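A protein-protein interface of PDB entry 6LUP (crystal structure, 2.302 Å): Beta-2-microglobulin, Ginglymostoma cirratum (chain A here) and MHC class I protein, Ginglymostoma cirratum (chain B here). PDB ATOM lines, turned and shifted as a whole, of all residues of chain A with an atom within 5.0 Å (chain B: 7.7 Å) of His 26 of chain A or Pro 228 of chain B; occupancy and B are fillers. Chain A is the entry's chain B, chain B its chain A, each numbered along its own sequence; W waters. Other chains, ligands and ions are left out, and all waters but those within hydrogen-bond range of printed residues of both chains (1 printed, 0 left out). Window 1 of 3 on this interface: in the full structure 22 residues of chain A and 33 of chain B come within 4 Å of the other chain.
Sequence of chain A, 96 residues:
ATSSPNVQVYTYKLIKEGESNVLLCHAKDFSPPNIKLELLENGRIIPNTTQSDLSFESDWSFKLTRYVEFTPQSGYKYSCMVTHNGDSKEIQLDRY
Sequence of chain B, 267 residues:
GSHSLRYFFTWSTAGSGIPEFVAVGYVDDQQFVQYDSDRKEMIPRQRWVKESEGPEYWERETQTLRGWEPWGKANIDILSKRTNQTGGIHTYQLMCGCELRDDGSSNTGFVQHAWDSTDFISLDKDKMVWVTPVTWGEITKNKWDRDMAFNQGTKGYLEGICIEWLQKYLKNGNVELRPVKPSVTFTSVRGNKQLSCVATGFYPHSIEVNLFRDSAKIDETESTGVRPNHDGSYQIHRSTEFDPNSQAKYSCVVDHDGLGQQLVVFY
Of the 12 printed residues of chain A, 5 touch a printed residue of chain B.
Printed residues of chain A that touch a printed residue of chain B: Gln 8, Tyr 10, Leu 24, His 26 and Thr 65.
Of the 14 printed residues of chain B, 5 touch a printed residue of chain A.
Printed residues of chain B that touch a printed residue of chain A: Arg 227, Pro 228, Asn 229, His 230 and Gln 235.
Hydrophobic or aromatic side chains of chain B that line the printed part of chain A: Pro 228.
Along chain B the printed residues that touch a printed residue of chain A span positions 227 to 235.
Among the printed residues, 9 pairs touch across the chains.
Cys 25 of chain A touches none of the printed residues of chain B.
His 26 of chain A touches one residue of chain B.
Thr 200 of chain B touches none of the printed residues of chain A.
Of the printed residues of chain A, Pro 228 of chain B touches Tyr 10 (2.7 Å), Leu 24 (3.7 Å), His 26 (3.3 Å) and Thr 65 (3.4 Å).
Of the printed residues of chain A, Asn 229 of chain B touches Leu 24 (3.5 Å).
Printed residues of chain A within 4 Å of His 230 of chain B: Leu 24.
Printed residues of chain A within 4 Å of Gln 235 of chain B: Tyr 10.
The nearest residue of chain B that does not touch His 26 of chain A is Arg 227 of chain B (4.7 Å).
The nearest printed residue of chain A that does not touch Gln 235 of chain B is Leu 24 of chain A (4.7 Å).
Water W1 lies within hydrogen-bond range of the side-chain amino group (NZ) of Lys 28 of chain A (2.7 Å), the backbone carbonyl oxygen (O) of Val 226 of chain B (2.9 Å) and the side-chain amide oxygen (OE1) of Gln 8 of chain A (3.0 Å).
The backbone carbonyl oxygen of Tyr 10 of chain A lies within hydrogen-bond range of the backbone NH of Leu 24 of chain A (2.8 Å).
A ring nitrogen (ND1) of His 26 of chain A sits at hydrogen-bond distance from the side-chain hydroxyl of Thr 65 of chain A (2.9 Å).
The side-chain hydroxyl (OG1) of Thr 200 of chain B sits at hydrogen-bond distance from the side-chain amide oxygen (OD1) of Asn 229 of chain B.
The side-chain amide oxygen (OD1) of Asn 229 of chain B lies close to the backbone carbonyl oxygen (O) of Tyr 234 of chain B, at 3.2 Å.
The backbone carbonyl oxygen of Arg 227 of chain B lies within hydrogen-bond range of the backbone NH of Gln 235 of chain B.
The side-chain amide oxygen of Asn 229 of chain B lies within hydrogen-bond range of the side-chain hydroxyl of Ser 233 of chain B (3.2 Å).
The side-chain hydroxyl (OH) of Tyr 10 of chain A is in hydrogen-bond range of the backbone carbonyl oxygen (O) of Pro 228 of chain B.
The side-chain amide nitrogen (NE2) of Gln 8 of chain A sits close to the guanidinium group (NH1) of Arg 227 of chain B.
CB of Tyr 10 of chain A touches NH2 of Arg 227 of chain B (3.4 Å).
CD2 of Tyr 10 of chain A touches NE2 of Gln 235 of chain B, 3.3 Å away.
Leu 24 of chain A touches Pro 228 of chain B (CD2 to O, 3.7 Å).
C of Asn 229 of chain B touches CD2 of Leu 24 of chain A (3.5 Å).
His 230 of chain B touches Leu 24 of chain A.
ND1 of His 26 of chain A touches CG of Pro 228 of chain B, at 3.3 Å.
Thr 65 of chain A touches Pro 228 of chain B (OG1 to CG, 3.4 Å).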
ATOM      1  N   ASN A   6      24.910  -5.932   9.981  1.00  0.00           N
ATOM      2  CA  ASN A   6      24.203  -5.001   9.124  1.00  0.00           C
ATOM      3  C   ASN A   6      23.588  -5.823   7.994  1.00  0.00           C
ATOM      4  O   ASN A   6      24.306  -6.483   7.242  1.00  0.00           O
ATOM      5  CB  ASN A   6      25.170  -3.955   8.572  1.00  0.00           C
ATOM      6  CG  ASN A   6      24.470  -2.877   7.765  1.00  0.00           C
ATOM      7  OD1 ASN A   6      23.981  -3.120   6.659  1.00  0.00           O
ATOM      8  ND2 ASN A   6      24.434  -1.669   8.312  1.00  0.00           N
ATOM      9  N   VAL A   7      22.262  -5.801   7.891  1.00  0.00           N
ATOM     10  CA  VAL A   7      21.552  -6.629   6.919  1.00  0.00           C
ATOM     11  C   VAL A   7      20.825  -5.780   5.882  1.00  0.00           C
ATOM     12  O   VAL A   7      20.109  -4.845   6.231  1.00  0.00           O
ATOM     13  CB  VAL A   7      20.526  -7.557   7.606  1.00  0.00           C
ATOM     14  CG1 VAL A   7      19.804  -8.422   6.581  1.00  0.00           C
ATOM     15  CG2 VAL A   7      21.203  -8.424   8.655  1.00  0.00           C
ATOM     16  N   GLN A   8      21.013  -6.118   4.610  1.00  0.00           N
ATOM     17  CA  GLN A   8      20.256  -5.506   3.523  1.00  0.00           C
ATOM     18  C   GLN A   8      19.528  -6.576   2.725  1.00  0.00           C
ATOM     19  O   GLN A   8      20.059  -7.666   2.508  1.00  0.00           O
ATOM     20  CB  GLN A   8      21.178  -4.710   2.604  1.00  0.00           C
ATOM     21  CG  GLN A   8      21.716  -3.437   3.222  1.00  0.00           C
ATOM     22  CD  GLN A   8      22.761  -2.774   2.358  1.00  0.00           C
ATOM     23  OE1 GLN A   8      23.931  -3.150   2.375  1.00  0.00           O
ATOM     24  NE2 GLN A   8      22.347  -1.772   1.602  1.00  0.00           N
ATOM     25  N   TYR A  10      17.495  -6.912  -1.018  1.00  0.00           N
ATOM     26  CA  TYR A  10      17.353  -6.176  -2.265  1.00  0.00           C
ATOM     27  C   TYR A  10      17.307  -7.124  -3.449  1.00  0.00           C
ATOM     28  O   TYR A  10      17.465  -8.333  -3.290  1.00  0.00           O
ATOM     29  CB  TYR A  10      18.518  -5.198  -2.421  1.00  0.00           C
ATOM     30  CG  TYR A  10      19.882  -5.833  -2.247  1.00  0.00           C
ATOM     31  CD1 TYR A  10      20.403  -6.078  -0.973  1.00  0.00           C
ATOM     32  CD2 TYR A  10      20.655  -6.183  -3.355  1.00  0.00           C
ATOM     33  CE1 TYR A  10      21.646  -6.657  -0.809  1.00  0.00           C
ATOM     34  CE2 TYR A  10      21.902  -6.760  -3.200  1.00  0.00           C
ATOM     35  CZ  TYR A  10      22.389  -6.996  -1.926  1.00  0.00           C
ATOM     36  OH  TYR A  10      23.630  -7.567  -1.766  1.00  0.00           O
ATOM     37  N   LEU A  24      18.127 -10.995  -3.012  1.00  0.00           N
ATOM     38  CA  LEU A  24      19.340 -11.103  -2.205  1.00  0.00           C
ATOM     39  C   LEU A  24      19.163 -10.613  -0.771  1.00  0.00           C
ATOM     40  O   LEU A  24      18.413  -9.668  -0.508  1.00  0.00           O
ATOM     41  CB  LEU A  24      20.485 -10.334  -2.858  1.00  0.00           C
ATOM     42  CG  LEU A  24      20.726 -10.631  -4.336  1.00  0.00           C
ATOM     43  CD1 LEU A  24      20.225  -9.476  -5.189  1.00  0.00           C
ATOM     44  CD2 LEU A  24      22.201 -10.891  -4.588  1.00  0.00           C
ATOM     45  N   CYS A  25      19.866 -11.270   0.143  1.00  0.00           N
ATOM     46  CA  CYS A  25      19.953 -10.864   1.537  1.00  0.00           C
ATOM     47  C   CYS A  25      21.431 -10.884   1.910  1.00  0.00           C
ATOM     48  O   CYS A  25      22.044 -11.953   1.984  1.00  0.00           O
ATOM     49  CB  CYS A  25      19.153 -11.822   2.423  1.00  0.00           C
ATOM     50  SG  CYS A  25      19.238 -11.512   4.205  1.00  0.00           S
ATOM     51  N   HIS A  26      22.007  -9.702   2.111  1.00  0.00           N
ATOM     52  CA  HIS A  26      23.429  -9.586   2.417  1.00  0.00           C
ATOM     53  C   HIS A  26      23.681  -9.127   3.850  1.00  0.00           C
ATOM     54  O   HIS A  26      23.191  -8.082   4.274  1.00  0.00           O
ATOM     55  CB  HIS A  26      24.119  -8.647   1.425  1.00  0.00           C
ATOM     56  CG  HIS A  26      25.570  -8.429   1.715  1.00  0.00           C
ATOM     57  ND1 HIS A  26      26.532  -9.379   1.451  1.00  0.00           N
ATOM     58  CD2 HIS A  26      26.222  -7.373   2.258  1.00  0.00           C
ATOM     59  CE1 HIS A  26      27.715  -8.916   1.814  1.00  0.00           C
ATOM     60  NE2 HIS A  26      27.555  -7.701   2.307  1.00  0.00           N
ATOM     61  N   ALA A  27      24.452  -9.916   4.587  1.00  0.00           N
ATOM     62  CA  ALA A  27      24.826  -9.574   5.950  1.00  0.00           C
ATOM     63  C   ALA A  27      26.298  -9.179   6.006  1.00  0.00           C
ATOM     64  O   ALA A  27      27.150  -9.856   5.417  1.00  0.00           O
ATOM     65  CB  ALA A  27      24.555 -10.745   6.877  1.00  0.00           C
ATOM     66  N   LYS A  28      26.595  -8.081   6.697  1.00  0.00           N
ATOM     67  CA  LYS A  28      27.977  -7.634   6.863  1.00  0.00           C
ATOM     68  C   LYS A  28      28.249  -7.074   8.259  1.00  0.00           C
ATOM     69  O   LYS A  28      27.326  -6.912   9.064  1.00  0.00           O
ATOM     70  CB  LYS A  28      28.372  -6.622   5.771  1.00  0.00           C
ATOM     71  CG  LYS A  28      27.672  -5.276   5.846  1.00  0.00           C
ATOM     72  CD  LYS A  28      28.128  -4.362   4.721  1.00  0.00           C
ATOM     73  CE  LYS A  28      27.609  -2.952   4.925  1.00  0.00           C
ATOM     74  NZ  LYS A  28      27.795  -2.116   3.710  1.00  0.00           N
ATOM     75  N   LYS A  63      31.113 -11.467   6.229  1.00  0.00           N
ATOM     76  CA  LYS A  63      30.116 -11.118   5.220  1.00  0.00           C
ATOM     77  C   LYS A  63      29.551 -12.384   4.592  1.00  0.00           C
ATOM     78  O   LYS A  63      30.291 -13.329   4.298  1.00  0.00           O
ATOM     79  CB  LYS A  63      30.684 -10.172   4.145  1.00  0.00           C
ATOM     80  CG  LYS A  63      31.947 -10.661   3.457  1.00  0.00           C
ATOM     81  CD  LYS A  63      32.428  -9.709   2.371  1.00  0.00           C
ATOM     82  CE  LYS A  63      33.797 -10.149   1.870  1.00  0.00           C
ATOM     83  NZ  LYS A  63      34.100  -9.729   0.472  1.00  0.00           N
ATOM     84  N   LEU A  64      28.235 -12.385   4.403  1.00  0.00           N
ATOM     85  CA  LEU A  64      27.510 -13.505   3.824  1.00  0.00           C
ATOM     86  C   LEU A  64      26.377 -13.012   2.947  1.00  0.00           C
ATOM     87  O   LEU A  64      25.775 -11.972   3.221  1.00  0.00           O
ATOM     88  CB  LEU A  64      26.906 -14.376   4.923  1.00  0.00           C
ATOM     89  CG  LEU A  64      27.520 -15.729   5.283  1.00  0.00           C
ATOM     90  CD1 LEU A  64      26.521 -16.490   6.139  1.00  0.00           C
ATOM     91  CD2 LEU A  64      27.897 -16.543   4.051  1.00  0.00           C
ATOM     92  N   THR A  65      26.064 -13.776   1.909  1.00  0.00           N
ATOM     93  CA  THR A  65      24.978 -13.424   1.013  1.00  0.00           C
ATOM     94  C   THR A  65      24.174 -14.677   0.693  1.00  0.00           C
ATOM     95  O   THR A  65      24.744 -15.717   0.353  1.00  0.00           O
ATOM     96  CB  THR A  65      25.514 -12.799  -0.295  1.00  0.00           C
ATOM     97  OG1 THR A  65      26.597 -11.913   0.007  1.00  0.00           O
ATOM     98  CG2 THR A  65      24.427 -12.031  -1.033  1.00  0.00           C
ATOM     99  N   THR B 200      24.512  -1.228 -11.335  1.00  0.00           N
ATOM    100  CA  THR B 200      24.476  -2.667 -11.093  1.00  0.00           C
ATOM    101  C   THR B 200      25.282  -3.433 -12.143  1.00  0.00           C
ATOM    102  O   THR B 200      25.560  -2.913 -13.228  1.00  0.00           O
ATOM    103  CB  THR B 200      23.021  -3.185 -11.025  1.00  0.00           C
ATOM    104  OG1 THR B 200      22.993  -4.476 -10.400  1.00  0.00           O
ATOM    105  CG2 THR B 200      22.388  -3.259 -12.415  1.00  0.00           C
ATOM    106  N   HIS B 205      34.512  -4.373  -7.346  1.00  0.00           N
ATOM    107  CA  HIS B 205      33.554  -3.718  -6.449  1.00  0.00           C
ATOM    108  C   HIS B 205      33.752  -2.205  -6.311  1.00  0.00           C
ATOM    109  O   HIS B 205      32.782  -1.462  -6.137  1.00  0.00           O
ATOM    110  CB  HIS B 205      33.588  -4.376  -5.064  1.00  0.00           C
ATOM    111  CG  HIS B 205      34.661  -3.842  -4.171  1.00  0.00           C
ATOM    112  ND1 HIS B 205      34.411  -2.913  -3.182  1.00  0.00           N
ATOM    113  CD2 HIS B 205      35.994  -4.080  -4.136  1.00  0.00           C
ATOM    114  CE1 HIS B 205      35.542  -2.611  -2.570  1.00  0.00           C
ATOM    115  NE2 HIS B 205      36.517  -3.306  -3.129  1.00  0.00           N
ATOM    116  N   GLY B 225      25.775   1.881  -0.200  1.00  0.00           N
ATOM    117  CA  GLY B 225      27.137   1.379  -0.290  1.00  0.00           C
ATOM    118  C   GLY B 225      27.168   0.246  -1.296  1.00  0.00           C
ATOM    119  O   GLY B 225      26.120  -0.258  -1.710  1.00  0.00           O
ATOM    120  N   VAL B 226      28.365  -0.155  -1.704  1.00  0.00           N
ATOM    121  CA  VAL B 226      28.504  -1.271  -2.634  1.00  0.00           C
ATOM    122  C   VAL B 226      28.078  -2.572  -1.938  1.00  0.00           C
ATOM    123  O   VAL B 226      28.387  -2.792  -0.765  1.00  0.00           O
ATOM    124  CB  VAL B 226      29.930  -1.340  -3.245  1.00  0.00           C
ATOM    125  CG1 VAL B 226      30.992  -1.476  -2.162  1.00  0.00           C
ATOM    126  CG2 VAL B 226      30.046  -2.472  -4.260  1.00  0.00           C
ATOM    127  N   ARG B 227      27.328  -3.404  -2.659  1.00  0.00           N
ATOM    128  CA  ARG B 227      26.874  -4.693  -2.145  1.00  0.00           C
ATOM    129  C   ARG B 227      26.852  -5.731  -3.265  1.00  0.00           C
ATOM    130  O   ARG B 227      26.650  -5.381  -4.427  1.00  0.00           O
ATOM    131  CB  ARG B 227      25.504  -4.570  -1.471  1.00  0.00           C
ATOM    132  CG  ARG B 227      24.428  -3.941  -2.338  1.00  0.00           C
ATOM    133  CD  ARG B 227      23.200  -3.580  -1.523  1.00  0.00           C
ATOM    134  NE  ARG B 227      22.120  -3.117  -2.386  1.00  0.00           N
ATOM    135  CZ  ARG B 227      20.968  -2.616  -1.952  1.00  0.00           C
ATOM    136  NH1 ARG B 227      20.731  -2.512  -0.649  1.00  0.00           N
ATOM    137  NH2 ARG B 227      20.048  -2.219  -2.823  1.00  0.00           N
ATOM    138  N   PRO B 228      27.079  -7.009  -2.916  1.00  0.00           N
ATOM    139  CA  PRO B 228      27.221  -8.057  -3.924  1.00  0.00           C
ATOM    140  C   PRO B 228      25.909  -8.420  -4.610  1.00  0.00           C
ATOM    141  O   PRO B 228      24.845  -8.378  -3.990  1.00  0.00           O
ATOM    142  CB  PRO B 228      27.735  -9.252  -3.117  1.00  0.00           C
ATOM    143  CG  PRO B 228      27.198  -9.023  -1.745  1.00  0.00           C
ATOM    144  CD  PRO B 228      27.232  -7.537  -1.547  1.00  0.00           C
ATOM    145  N   ASN B 229      26.007  -8.759  -5.892  1.00  0.00           N
ATOM    146  CA  ASN B 229      24.935  -9.427  -6.607  1.00  0.00           C
ATOM    147  C   ASN B 229      25.095 -10.943  -6.475  1.00  0.00           C
ATOM    148  O   ASN B 229      25.790 -11.419  -5.577  1.00  0.00           O
ATOM    149  CB  ASN B 229      24.908  -8.987  -8.073  1.00  0.00           C
ATOM    150  CG  ASN B 229      24.364  -7.580  -8.250  1.00  0.00           C
ATOM    151  OD1 ASN B 229      24.923  -6.777  -8.991  1.00  0.00           O
ATOM    152  ND2 ASN B 229      23.266  -7.280  -7.570  1.00  0.00           N
ATOM    153  N   HIS B 230      24.442 -11.698  -7.355  1.00  0.00           N
ATOM    154  CA  HIS B 230      24.486 -13.160  -7.303  1.00  0.00           C
ATOM    155  C   HIS B 230      25.585 -13.788  -8.174  1.00  0.00           C
ATOM    156  O   HIS B 230      25.890 -14.970  -8.032  1.00  0.00           O
ATOM    157  CB  HIS B 230      23.127 -13.726  -7.712  1.00  0.00           C
ATOM    158  CG  HIS B 230      22.808 -13.533  -9.163  1.00  0.00           C
ATOM    159  ND1 HIS B 230      22.804 -12.292  -9.764  1.00  0.00           N
ATOM    160  CD2 HIS B 230      22.489 -14.422 -10.132  1.00  0.00           C
ATOM    161  CE1 HIS B 230      22.497 -12.425 -11.041  1.00  0.00           C
ATOM    162  NE2 HIS B 230      22.301 -13.708 -11.290  1.00  0.00           N
ATOM    163  N   ASP B 231      26.177 -12.998  -9.065  1.00  0.00           N
ATOM    164  CA  ASP B 231      27.015 -13.532 -10.137  1.00  0.00           C
ATOM    165  C   ASP B 231      28.437 -12.982 -10.126  1.00  0.00           C
ATOM    166  O   ASP B 231      29.073 -12.874 -11.177  1.00  0.00           O
ATOM    167  CB  ASP B 231      26.365 -13.225 -11.492  1.00  0.00           C
ATOM    168  CG  ASP B 231      26.129 -11.726 -11.711  1.00  0.00           C
ATOM    169  OD1 ASP B 231      26.478 -10.907 -10.829  1.00  0.00           O
ATOM    170  OD2 ASP B 231      25.589 -11.366 -12.775  1.00  0.00           O
ATOM    171  N   GLY B 232      28.929 -12.618  -8.945  1.00  0.00           N
ATOM    172  CA  GLY B 232      30.263 -12.046  -8.821  1.00  0.00           C
ATOM    173  C   GLY B 232      30.333 -10.549  -9.087  1.00  0.00           C
ATOM    174  O   GLY B 232      31.374  -9.928  -8.874  1.00  0.00           O
ATOM    175  N   SER B 233      29.235  -9.962  -9.555  1.00  0.00           N
ATOM    176  CA  SER B 233      29.186  -8.516  -9.784  1.00  0.00           C
ATOM    177  C   SER B 233      28.654  -7.778  -8.553  1.00  0.00           C
ATOM    178  O   SER B 233      28.243  -8.406  -7.573  1.00  0.00           O
ATOM    179  CB  SER B 233      28.360  -8.182 -11.031  1.00  0.00           C
ATOM    180  OG  SER B 233      26.977  -8.383 -10.805  1.00  0.00           O
ATOM    181  N   TYR B 234      28.674  -6.447  -8.605  1.00  0.00           N
ATOM    182  CA  TYR B 234      28.257  -5.615  -7.476  1.00  0.00           C
ATOM    183  C   TYR B 234      27.229  -4.564  -7.887  1.00  0.00           C
ATOM    184  O   TYR B 234      27.032  -4.307  -9.075  1.00  0.00           O
ATOM    185  CB  TYR B 234      29.480  -4.958  -6.824  1.00  0.00           C
ATOM    186  CG  TYR B 234      30.517  -5.960  -6.368  1.00  0.00           C
ATOM    187  CD1 TYR B 234      31.477  -6.452  -7.257  1.00  0.00           C
ATOM    188  CD2 TYR B 234      30.520  -6.444  -5.060  1.00  0.00           C
ATOM    189  CE1 TYR B 234      32.415  -7.386  -6.855  1.00  0.00           C
ATOM    190  CE2 TYR B 234      31.459  -7.379  -4.646  1.00  0.00           C
ATOM    191  CZ  TYR B 234      32.404  -7.846  -5.549  1.00  0.00           C
ATOM    192  OH  TYR B 234      33.341  -8.771  -5.155  1.00  0.00           O
ATOM    193  N   GLN B 235      26.574  -3.971  -6.893  1.00  0.00           N
ATOM    194  CA  GLN B 235      25.593  -2.912  -7.120  1.00  0.00           C
ATOM    195  C   GLN B 235      25.664  -1.841  -6.033  1.00  0.00           C
ATOM    196  O   GLN B 235      26.183  -2.082  -4.939  1.00  0.00           O
ATOM    197  CB  GLN B 235      24.169  -3.482  -7.219  1.00  0.00           C
ATOM    198  CG  GLN B 235      23.637  -4.095  -5.932  1.00  0.00           C
ATOM    199  CD  GLN B 235      22.137  -4.321  -5.961  1.00  0.00           C
ATOM    200  OE1 GLN B 235      21.641  -5.215  -6.648  1.00  0.00           O
ATOM    201  NE2 GLN B 235      21.409  -3.516  -5.204  1.00  0.00           N
ATOM    202  N   ILE B 236      25.145  -0.658  -6.351  1.00  0.00           N
ATOM    203  CA  ILE B 236      25.070   0.443  -5.395  1.00  0.00           C
ATOM    204  C   ILE B 236      23.921   1.385  -5.750  1.00  0.00           C
ATOM    205  O   ILE B 236      23.642   1.631  -6.928  1.00  0.00           O
ATOM    206  CB  ILE B 236      26.413   1.215  -5.284  1.00  0.00           C
ATOM    207  CG1 ILE B 236      26.330   2.289  -4.188  1.00  0.00           C
ATOM    208  CG2 ILE B 236      26.845   1.780  -6.635  1.00  0.00           C
ATOM    209  CD1 ILE B 236      27.668   2.870  -3.775  1.00  0.00           C
HETATM  210  O   HOH W   1      26.520  -2.050   1.331  1.00  0.00           O
